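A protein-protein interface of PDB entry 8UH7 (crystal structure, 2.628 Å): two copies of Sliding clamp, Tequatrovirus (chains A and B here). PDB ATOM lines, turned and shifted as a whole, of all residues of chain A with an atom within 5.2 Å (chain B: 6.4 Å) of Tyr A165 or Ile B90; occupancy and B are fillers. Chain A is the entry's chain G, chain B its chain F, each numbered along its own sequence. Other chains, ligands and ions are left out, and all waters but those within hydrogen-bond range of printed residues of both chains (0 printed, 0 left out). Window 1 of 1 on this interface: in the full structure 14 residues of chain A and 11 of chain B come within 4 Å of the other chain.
Among the printed residues, merely in contact across the chains: Gln A125 with Val B67 (3.5 Å), Gln A125 with Asp B85 (3.98 Å), Leu A133 with Ile B63 (3.5 Å), Leu A133 with Phe B91 (3.7 Å), Val A163 with Phe B91 (3.3 Å), Lys A164 with Ile B90 (3.8 Å), Tyr A165 with Ser B88 (3.5 Å), Tyr A165 with Thr B89 (3.5 Å), Tyr A165 with Ile B90 (3.8 Å), Ser A166 with Ser B88 (3.2 Å) and Leu A167 with Arg B87 (3.8 Å).
Of the 13 printed residues of chain B, 8 touch a printed residue of chain A. Printed residues of chain B that touch a printed residue of chain A: Ile B63, Val B67, Asp B85, Arg B87, Ser B88, Thr B89, Ile B90 and Phe B91. Hydrophobic or aromatic side chains of chain B within 4 Å of the printed part of chain A: Ile B63, Val B67, Ile B90 and Phe B91. Hydrophobic or aromatic side chains of chain A within 4 Å of the printed part of chain B: Leu A133 and Tyr A165. Along chain A the printed residues that touch a printed residue of chain B span positions 122 to 167. Among the printed residues, 15 pairs touch across the chains. Among the printed residues, Asp or Glu carboxylates within 4 Å of a Lys or Arg side-chain nitrogen of the other chain: Asp A122 with Arg B87.
Printed residues of chain B within 4 Å of Gln A125: Val B67, Asp B85 and Ser B88. Of the printed residues of chain B, Lys A164 touches Ile B90 (3.8 Å) and Phe B91 (2.9 Å). Tyr A165 touches just these residues of chain B: Ser B88 (3.5 Å), Thr B89 (3.5 Å) and Ile B90 (3.8 Å). Ala B84 touches none of the printed residues of chain A. Of chain A, only Lys A164 (3.8 Å) and Tyr A165 (3.8 Å) come within 4 Å of Ile B90. Trp B92 touches none of the printed residues of chain A. The nearest residue of chain B that does not touch Tyr A165 is Phe B91 (4.8 Å). The nearest printed residue of chain B that does not touch Leu A133 is Ile B90 (4.1 Å).
NE of Arg B87 lies within salt-bridge range of OD2 of Asp A122 (3.5 Å). NE2 of Gln A125 sits at hydrogen-bond distance from OG of Ser B88, at 2.6 Å. The backbone NH (N) of Thr B89 sits at hydrogen-bond distance from the backbone carbonyl oxygen (O) of Ser A166, at 2.7 Å. N of Phe B91 sits at hydrogen-bond distance from O of Lys A164, 2.9 Å away.
No position is printed for both chains. Of the 15 pairs that touch across the chains among the printed residues, none has its exchanged pair printed and touching as well.
O of Ile B90 sits at hydrogen-bond distance from N of Ile B83, at 2.9 Å. The side-chain amide oxygen (OE1) of Gln A125 is in hydrogen-bond range of the side-chain hydroxyl (OH) of Tyr A165, at 3.0 Å. The backbone NH of Ile A149 lies within hydrogen-bond range of the backbone carbonyl oxygen of Leu A167 (2.9 Å). The side-chain amide oxygen (OD1) of Asn A150 lies within hydrogen-bond range of the side-chain hydroxyl (OG) of Ser A166, 3.4 Å away. The backbone carbonyl oxygen (O) of Gly A151 lies within hydrogen-bond range of the backbone NH (N) of Lys A164 (2.9 Å). The backbone NH (N) of Gly A151 sits at hydrogen-bond distance from the backbone carbonyl oxygen (O) of Tyr A165, at 2.8 Å.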
ATOM      1  N   ASP A 122     -10.081   9.497  20.450  1.00  0.00           N
ATOM      2  CA  ASP A 122      -9.548  10.016  19.194  1.00  0.00           C
ATOM      3  C   ASP A 122      -8.214  10.718  19.413  1.00  0.00           C
ATOM      4  O   ASP A 122      -7.289  10.578  18.606  1.00  0.00           O
ATOM      5  CB  ASP A 122     -10.555  10.966  18.545  1.00  0.00           C
ATOM      6  CG  ASP A 122     -11.806  10.254  18.060  1.00  0.00           C
ATOM      7  OD1 ASP A 122     -11.737   9.030  17.809  1.00  0.00           O
ATOM      8  OD2 ASP A 122     -12.857  10.917  17.924  1.00  0.00           O
ATOM      9  N   GLN A 125      -5.541   8.052  20.033  1.00  0.00           N
ATOM     10  CA  GLN A 125      -5.198   7.419  18.765  1.00  0.00           C
ATOM     11  C   GLN A 125      -4.335   8.337  17.914  1.00  0.00           C
ATOM     12  O   GLN A 125      -3.377   7.884  17.281  1.00  0.00           O
ATOM     13  CB  GLN A 125      -6.462   7.027  18.003  1.00  0.00           C
ATOM     14  CG  GLN A 125      -6.175   6.346  16.675  1.00  0.00           C
ATOM     15  CD  GLN A 125      -7.358   6.375  15.734  1.00  0.00           C
ATOM     16  OE1 GLN A 125      -8.217   7.252  15.824  1.00  0.00           O
ATOM     17  NE2 GLN A 125      -7.411   5.411  14.821  1.00  0.00           N
ATOM     18  N   LEU A 126      -4.663   9.631  17.887  1.00  0.00           N
ATOM     19  CA  LEU A 126      -3.856  10.583  17.133  1.00  0.00           C
ATOM     20  C   LEU A 126      -2.426  10.626  17.654  1.00  0.00           C
ATOM     21  O   LEU A 126      -1.475  10.611  16.868  1.00  0.00           O
ATOM     22  CB  LEU A 126      -4.491  11.972  17.194  1.00  0.00           C
ATOM     23  CG  LEU A 126      -3.644  13.128  16.658  1.00  0.00           C
ATOM     24  CD1 LEU A 126      -3.262  12.899  15.204  1.00  0.00           C
ATOM     25  CD2 LEU A 126      -4.384  14.442  16.817  1.00  0.00           C
ATOM     26  N   VAL A 129      -0.610   7.280  16.790  1.00  0.00           N
ATOM     27  CA  VAL A 129      -0.310   7.242  15.364  1.00  0.00           C
ATOM     28  C   VAL A 129       0.801   8.228  15.027  1.00  0.00           C
ATOM     29  O   VAL A 129       1.648   7.961  14.166  1.00  0.00           O
ATOM     30  CB  VAL A 129      -1.593   7.513  14.556  1.00  0.00           C
ATOM     31  CG1 VAL A 129      -1.266   7.923  13.134  1.00  0.00           C
ATOM     32  CG2 VAL A 129      -2.485   6.282  14.563  1.00  0.00           C
ATOM     33  N   LEU A 133       3.499   6.797  12.565  1.00  0.00           N
ATOM     34  CA  LEU A 133       3.839   7.347  11.256  1.00  0.00           C
ATOM     35  C   LEU A 133       4.796   8.526  11.333  1.00  0.00           C
ATOM     36  O   LEU A 133       5.188   9.043  10.280  1.00  0.00           O
ATOM     37  CB  LEU A 133       2.573   7.769  10.508  1.00  0.00           C
ATOM     38  CG  LEU A 133       1.746   6.651   9.874  1.00  0.00           C
ATOM     39  CD1 LEU A 133       0.726   6.122  10.852  1.00  0.00           C
ATOM     40  CD2 LEU A 133       1.067   7.129   8.603  1.00  0.00           C
ATOM     41  N   ILE A 135       4.320  11.604  12.176  1.00  0.00           N
ATOM     42  CA  ILE A 135       3.769  12.864  11.692  1.00  0.00           C
ATOM     43  C   ILE A 135       4.076  13.954  12.708  1.00  0.00           C
ATOM     44  O   ILE A 135       3.963  13.748  13.923  1.00  0.00           O
ATOM     45  CB  ILE A 135       2.256  12.739  11.416  1.00  0.00           C
ATOM     46  CG1 ILE A 135       1.480  12.376  12.682  1.00  0.00           C
ATOM     47  CG2 ILE A 135       1.987  11.714  10.325  1.00  0.00           C
ATOM     48  CD1 ILE A 135       0.746  13.545  13.305  1.00  0.00           C
ATOM     49  N   ILE A 149      -9.011  16.285  10.952  1.00  0.00           N
ATOM     50  CA  ILE A 149      -7.627  16.532  11.326  1.00  0.00           C
ATOM     51  C   ILE A 149      -6.764  15.678  10.410  1.00  0.00           C
ATOM     52  O   ILE A 149      -6.837  14.444  10.452  1.00  0.00           O
ATOM     53  CB  ILE A 149      -7.369  16.198  12.801  1.00  0.00           C
ATOM     54  CG1 ILE A 149      -8.076  17.200  13.715  1.00  0.00           C
ATOM     55  CG2 ILE A 149      -5.875  16.146  13.085  1.00  0.00           C
ATOM     56  CD1 ILE A 149      -7.932  16.880  15.189  1.00  0.00           C
ATOM     57  N   ASN A 150      -5.968  16.324   9.565  1.00  0.00           N
ATOM     58  CA  ASN A 150      -5.024  15.632   8.699  1.00  0.00           C
ATOM     59  C   ASN A 150      -3.628  15.701   9.304  1.00  0.00           C
ATOM     60  O   ASN A 150      -3.191  16.758   9.761  1.00  0.00           O
ATOM     61  CB  ASN A 150      -5.017  16.236   7.294  1.00  0.00           C
ATOM     62  CG  ASN A 150      -6.310  15.988   6.545  1.00  0.00           C
ATOM     63  OD1 ASN A 150      -7.040  15.044   6.841  1.00  0.00           O
ATOM     64  ND2 ASN A 150      -6.596  16.834   5.562  1.00  0.00           N
ATOM     65  N   GLY A 151      -2.933  14.570   9.307  1.00  0.00           N
ATOM     66  CA  GLY A 151      -1.624  14.479   9.919  1.00  0.00           C
ATOM     67  C   GLY A 151      -0.522  14.238   8.910  1.00  0.00           C
ATOM     68  O   GLY A 151      -0.526  13.215   8.209  1.00  0.00           O
ATOM     69  N   VAL A 163      -1.047  13.282   2.848  1.00  0.00           N
ATOM     70  CA  VAL A 163      -1.726  13.039   4.116  1.00  0.00           C
ATOM     71  C   VAL A 163      -1.382  11.641   4.614  1.00  0.00           C
ATOM     72  O   VAL A 163      -1.692  10.639   3.958  1.00  0.00           O
ATOM     73  CB  VAL A 163      -3.241  13.210   3.959  1.00  0.00           C
ATOM     74  CG1 VAL A 163      -3.957  12.766   5.219  1.00  0.00           C
ATOM     75  CG2 VAL A 163      -3.580  14.651   3.629  1.00  0.00           C
ATOM     76  N   LYS A 164      -0.750  11.568   5.784  1.00  0.00           N
ATOM     77  CA  LYS A 164      -0.422  10.283   6.386  1.00  0.00           C
ATOM     78  C   LYS A 164      -1.481   9.801   7.368  1.00  0.00           C
ATOM     79  O   LYS A 164      -1.662   8.588   7.521  1.00  0.00           O
ATOM     80  CB  LYS A 164       0.939  10.354   7.088  1.00  0.00           C
ATOM     81  CG  LYS A 164       2.120  10.380   6.131  1.00  0.00           C
ATOM     82  CD  LYS A 164       2.059   9.199   5.170  1.00  0.00           C
ATOM     83  CE  LYS A 164       2.504   9.591   3.767  1.00  0.00           C
ATOM     84  NZ  LYS A 164       2.237   8.504   2.783  1.00  0.00           N
ATOM     85  N   TYR A 165      -2.187  10.710   8.036  1.00  0.00           N
ATOM     86  CA  TYR A 165      -3.255  10.319   8.949  1.00  0.00           C
ATOM     87  C   TYR A 165      -4.475  11.196   8.716  1.00  0.00           C
ATOM     88  O   TYR A 165      -4.353  12.347   8.301  1.00  0.00           O
ATOM     89  CB  TYR A 165      -2.797  10.419  10.411  1.00  0.00           C
ATOM     90  CG  TYR A 165      -3.869  10.136  11.440  1.00  0.00           C
ATOM     91  CD1 TYR A 165      -4.290   8.838  11.697  1.00  0.00           C
ATOM     92  CD2 TYR A 165      -4.443  11.166  12.171  1.00  0.00           C
ATOM     93  CE1 TYR A 165      -5.261   8.576  12.648  1.00  0.00           C
ATOM     94  CE2 TYR A 165      -5.417  10.914  13.122  1.00  0.00           C
ATOM     95  CZ  TYR A 165      -5.822   9.619  13.356  1.00  0.00           C
ATOM     96  OH  TYR A 165      -6.788   9.368  14.303  1.00  0.00           O
ATOM     97  N   SER A 166      -5.655  10.651   8.989  1.00  0.00           N
ATOM     98  CA  SER A 166      -6.875  11.437   8.845  1.00  0.00           C
ATOM     99  C   SER A 166      -7.873  11.020   9.912  1.00  0.00           C
ATOM    100  O   SER A 166      -8.111   9.825  10.112  1.00  0.00           O
ATOM    101  CB  SER A 166      -7.485  11.271   7.451  1.00  0.00           C
ATOM    102  OG  SER A 166      -8.630  12.095   7.306  1.00  0.00           O
ATOM    103  N   LEU A 167      -8.447  12.008  10.593  1.00  0.00           N
ATOM    104  CA  LEU A 167      -9.438  11.780  11.635  1.00  0.00           C
ATOM    105  C   LEU A 167     -10.643  12.667  11.370  1.00  0.00           C
ATOM    106  O   LEU A 167     -10.491  13.813  10.944  1.00  0.00           O
ATOM    107  CB  LEU A 167      -8.857  12.078  13.024  1.00  0.00           C
ATOM    108  CG  LEU A 167      -9.811  12.066  14.217  1.00  0.00           C
ATOM    109  CD1 LEU A 167     -10.437  10.693  14.385  1.00  0.00           C
ATOM    110  CD2 LEU A 167      -9.089  12.491  15.488  1.00  0.00           C
ATOM    111  N   ILE B  63       0.758  -0.114  13.552  1.00  0.00           N
ATOM    112  CA  ILE B  63      -0.310   0.806  13.179  1.00  0.00           C
ATOM    113  C   ILE B  63      -1.625   0.056  13.021  1.00  0.00           C
ATOM    114  O   ILE B  63      -2.694   0.568  13.376  1.00  0.00           O
ATOM    115  CB  ILE B  63       0.074   1.578  11.902  1.00  0.00           C
ATOM    116  CG1 ILE B  63       0.665   2.941  12.268  1.00  0.00           C
ATOM    117  CG2 ILE B  63      -1.122   1.740  10.969  1.00  0.00           C
ATOM    118  CD1 ILE B  63       1.923   2.877  13.109  1.00  0.00           C
ATOM    119  N   VAL B  67      -5.464   0.624  15.398  1.00  0.00           N
ATOM    120  CA  VAL B  67      -6.857   0.801  15.000  1.00  0.00           C
ATOM    121  C   VAL B  67      -7.651  -0.438  15.393  1.00  0.00           C
ATOM    122  O   VAL B  67      -7.114  -1.364  16.011  1.00  0.00           O
ATOM    123  CB  VAL B  67      -6.983   1.088  13.491  1.00  0.00           C
ATOM    124  CG1 VAL B  67      -6.448   2.475  13.170  1.00  0.00           C
ATOM    125  CG2 VAL B  67      -6.249   0.033  12.681  1.00  0.00           C
ATOM    126  N   ILE B  81      -1.045   2.332   0.851  1.00  0.00           N
ATOM    127  CA  ILE B  81      -1.951   1.427   1.554  1.00  0.00           C
ATOM    128  C   ILE B  81      -2.874   2.263   2.428  1.00  0.00           C
ATOM    129  O   ILE B  81      -2.413   2.972   3.331  1.00  0.00           O
ATOM    130  CB  ILE B  81      -1.185   0.397   2.399  1.00  0.00           C
ATOM    131  CG1 ILE B  81      -0.404  -0.564   1.498  1.00  0.00           C
ATOM    132  CG2 ILE B  81      -2.143  -0.358   3.315  1.00  0.00           C
ATOM    133  CD1 ILE B  81       0.440  -1.569   2.260  1.00  0.00           C
ATOM    134  N   LYS B  82      -4.175   2.181   2.164  1.00  0.00           N
ATOM    135  CA  LYS B  82      -5.175   2.848   2.983  1.00  0.00           C
ATOM    136  C   LYS B  82      -5.701   1.879   4.033  1.00  0.00           C
ATOM    137  O   LYS B  82      -6.001   0.719   3.724  1.00  0.00           O
ATOM    138  CB  LYS B  82      -6.327   3.375   2.123  1.00  0.00           C
ATOM    139  CG  LYS B  82      -7.464   3.987   2.933  1.00  0.00           C
ATOM    140  CD  LYS B  82      -8.595   4.500   2.051  1.00  0.00           C
ATOM    141  CE  LYS B  82      -8.143   5.661   1.179  1.00  0.00           C
ATOM    142  NZ  LYS B  82      -9.277   6.249   0.412  1.00  0.00           N
ATOM    143  N   ILE B  83      -5.799   2.354   5.271  1.00  0.00           N
ATOM    144  CA  ILE B  83      -6.350   1.589   6.383  1.00  0.00           C
ATOM    145  C   ILE B  83      -7.497   2.420   6.941  1.00  0.00           C
ATOM    146  O   ILE B  83      -7.275   3.428   7.622  1.00  0.00           O
ATOM    147  CB  ILE B  83      -5.301   1.284   7.457  1.00  0.00           C
ATOM    148  CG1 ILE B  83      -4.097   0.580   6.826  1.00  0.00           C
ATOM    149  CG2 ILE B  83      -5.913   0.440   8.572  1.00  0.00           C
ATOM    150  CD1 ILE B  83      -2.944   0.368   7.775  1.00  0.00           C
ATOM    151  N   ALA B  84      -8.724   2.009   6.642  1.00  0.00           N
ATOM    152  CA  ALA B  84      -9.924   2.729   7.039  1.00  0.00           C
ATOM    153  C   ALA B  84     -10.481   2.140   8.328  1.00  0.00           C
ATOM    154  O   ALA B  84     -10.612   0.919   8.456  1.00  0.00           O
ATOM    155  CB  ALA B  84     -10.981   2.674   5.935  1.00  0.00           C
ATOM    156  N   ASP B  85     -10.801   3.015   9.276  1.00  0.00           N
ATOM    157  CA  ASP B  85     -11.431   2.658  10.531  1.00  0.00           C
ATOM    158  C   ASP B  85     -12.827   3.288  10.566  1.00  0.00           C
ATOM    159  O   ASP B  85     -13.350   3.722   9.529  1.00  0.00           O
ATOM    160  CB  ASP B  85     -10.532   3.105  11.690  1.00  0.00           C
ATOM    161  CG  ASP B  85     -10.830   2.368  12.982  1.00  0.00           C
ATOM    162  OD1 ASP B  85     -11.680   1.453  12.964  1.00  0.00           O
ATOM    163  OD2 ASP B  85     -10.214   2.706  14.015  1.00  0.00           O
ATOM    164  N   ARG B  87     -13.823   6.183  12.238  1.00  0.00           N
ATOM    165  CA  ARG B  87     -13.692   7.618  12.039  1.00  0.00           C
ATOM    166  C   ARG B  87     -12.311   8.052  11.575  1.00  0.00           C
ATOM    167  O   ARG B  87     -12.173   9.181  11.093  1.00  0.00           O
ATOM    168  CB  ARG B  87     -14.032   8.370  13.336  1.00  0.00           C
ATOM    169  CG  ARG B  87     -15.344   7.944  13.971  1.00  0.00           C
ATOM    170  CD  ARG B  87     -15.409   8.349  15.434  1.00  0.00           C
ATOM    171  NE  ARG B  87     -15.297   9.793  15.611  1.00  0.00           N
ATOM    172  CZ  ARG B  87     -16.333  10.626  15.622  1.00  0.00           C
ATOM    173  NH1 ARG B  87     -17.565  10.160  15.464  1.00  0.00           N
ATOM    174  NH2 ARG B  87     -16.138  11.927  15.789  1.00  0.00           N
ATOM    175  N   SER B  88     -11.297   7.202  11.702  1.00  0.00           N
ATOM    176  CA  SER B  88      -9.925   7.541  11.361  1.00  0.00           C
ATOM    177  C   SER B  88      -9.466   6.763  10.134  1.00  0.00           C
ATOM    178  O   SER B  88     -10.050   5.742   9.761  1.00  0.00           O
ATOM    179  CB  SER B  88      -8.986   7.263  12.541  1.00  0.00           C
ATOM    180  OG  SER B  88      -9.112   5.924  12.988  1.00  0.00           O
ATOM    181  N   THR B  89      -8.401   7.261   9.507  1.00  0.00           N
ATOM    182  CA  THR B  89      -7.843   6.638   8.313  1.00  0.00           C
ATOM    183  C   THR B  89      -6.334   6.832   8.309  1.00  0.00           C
ATOM    184  O   THR B  89      -5.847   7.937   8.565  1.00  0.00           O
ATOM    185  CB  THR B  89      -8.458   7.227   7.038  1.00  0.00           C
ATOM    186  OG1 THR B  89      -9.888   7.194   7.134  1.00  0.00           O
ATOM    187  CG2 THR B  89      -8.026   6.427   5.820  1.00  0.00           C
ATOM    188  N   ILE B  90      -5.603   5.758   8.019  1.00  0.00           N
ATOM    189  CA  ILE B  90      -4.145   5.763   7.985  1.00  0.00           C
ATOM    190  C   ILE B  90      -3.695   5.535   6.548  1.00  0.00           C
ATOM    191  O   ILE B  90      -4.296   4.740   5.819  1.00  0.00           O
ATOM    192  CB  ILE B  90      -3.555   4.696   8.933  1.00  0.00           C
ATOM    193  CG1 ILE B  90      -3.577   5.182  10.387  1.00  0.00           C
ATOM    194  CG2 ILE B  90      -2.136   4.311   8.525  1.00  0.00           C
ATOM    195  CD1 ILE B  90      -4.932   5.099  11.061  1.00  0.00           C
ATOM    196  N   PHE B  91      -2.649   6.246   6.134  1.00  0.00           N
ATOM    197  CA  PHE B  91      -2.078   6.106   4.796  1.00  0.00           C
ATOM    198  C   PHE B  91      -0.633   5.636   4.946  1.00  0.00           C
ATOM    199  O   PHE B  91       0.290   6.448   5.040  1.00  0.00           O
ATOM    200  CB  PHE B  91      -2.167   7.418   4.019  1.00  0.00           C
ATOM    201  CG  PHE B  91      -3.568   7.802   3.631  1.00  0.00           C
ATOM    202  CD1 PHE B  91      -4.453   8.302   4.573  1.00  0.00           C
ATOM    203  CD2 PHE B  91      -3.994   7.679   2.319  1.00  0.00           C
ATOM    204  CE1 PHE B  91      -5.740   8.662   4.216  1.00  0.00           C
ATOM    205  CE2 PHE B  91      -5.279   8.036   1.955  1.00  0.00           C
ATOM    206  CZ  PHE B  91      -6.153   8.529   2.906  1.00  0.00           C
ATOM    207  N   TRP B  92      -0.441   4.320   4.966  1.00  0.00           N
ATOM    208  CA  TRP B  92       0.909   3.786   5.078  1.00  0.00           C
ATOM    209  C   TRP B  92       1.575   3.752   3.703  1.00  0.00           C
ATOM    210  O   TRP B  92       0.944   3.359   2.717  1.00  0.00           O
ATOM    211  CB  TRP B  92       0.888   2.386   5.681  1.00  0.00           C
ATOM    212  CG  TRP B  92       2.249   1.869   6.009  1.00  0.00           C
ATOM    213  CD1 TRP B  92       3.077   1.160   5.191  1.00  0.00           C
ATOM    214  CD2 TRP B  92       2.951   2.033   7.247  1.00  0.00           C
ATOM    215  NE1 TRP B  92       4.251   0.868   5.843  1.00  0.00           N
ATOM    216  CE2 TRP B  92       4.198   1.393   7.107  1.00  0.00           C
ATOM    217  CE3 TRP B  92       2.645   2.657   8.460  1.00  0.00           C
ATOM    218  CZ2 TRP B  92       5.138   1.358   8.134  1.00  0.00           C
ATOM    219  CZ3 TRP B  92       3.580   2.622   9.477  1.00  0.00           C
ATOM    220  CH2 TRP B  92       4.810   1.977   9.308  1.00  0.00           C
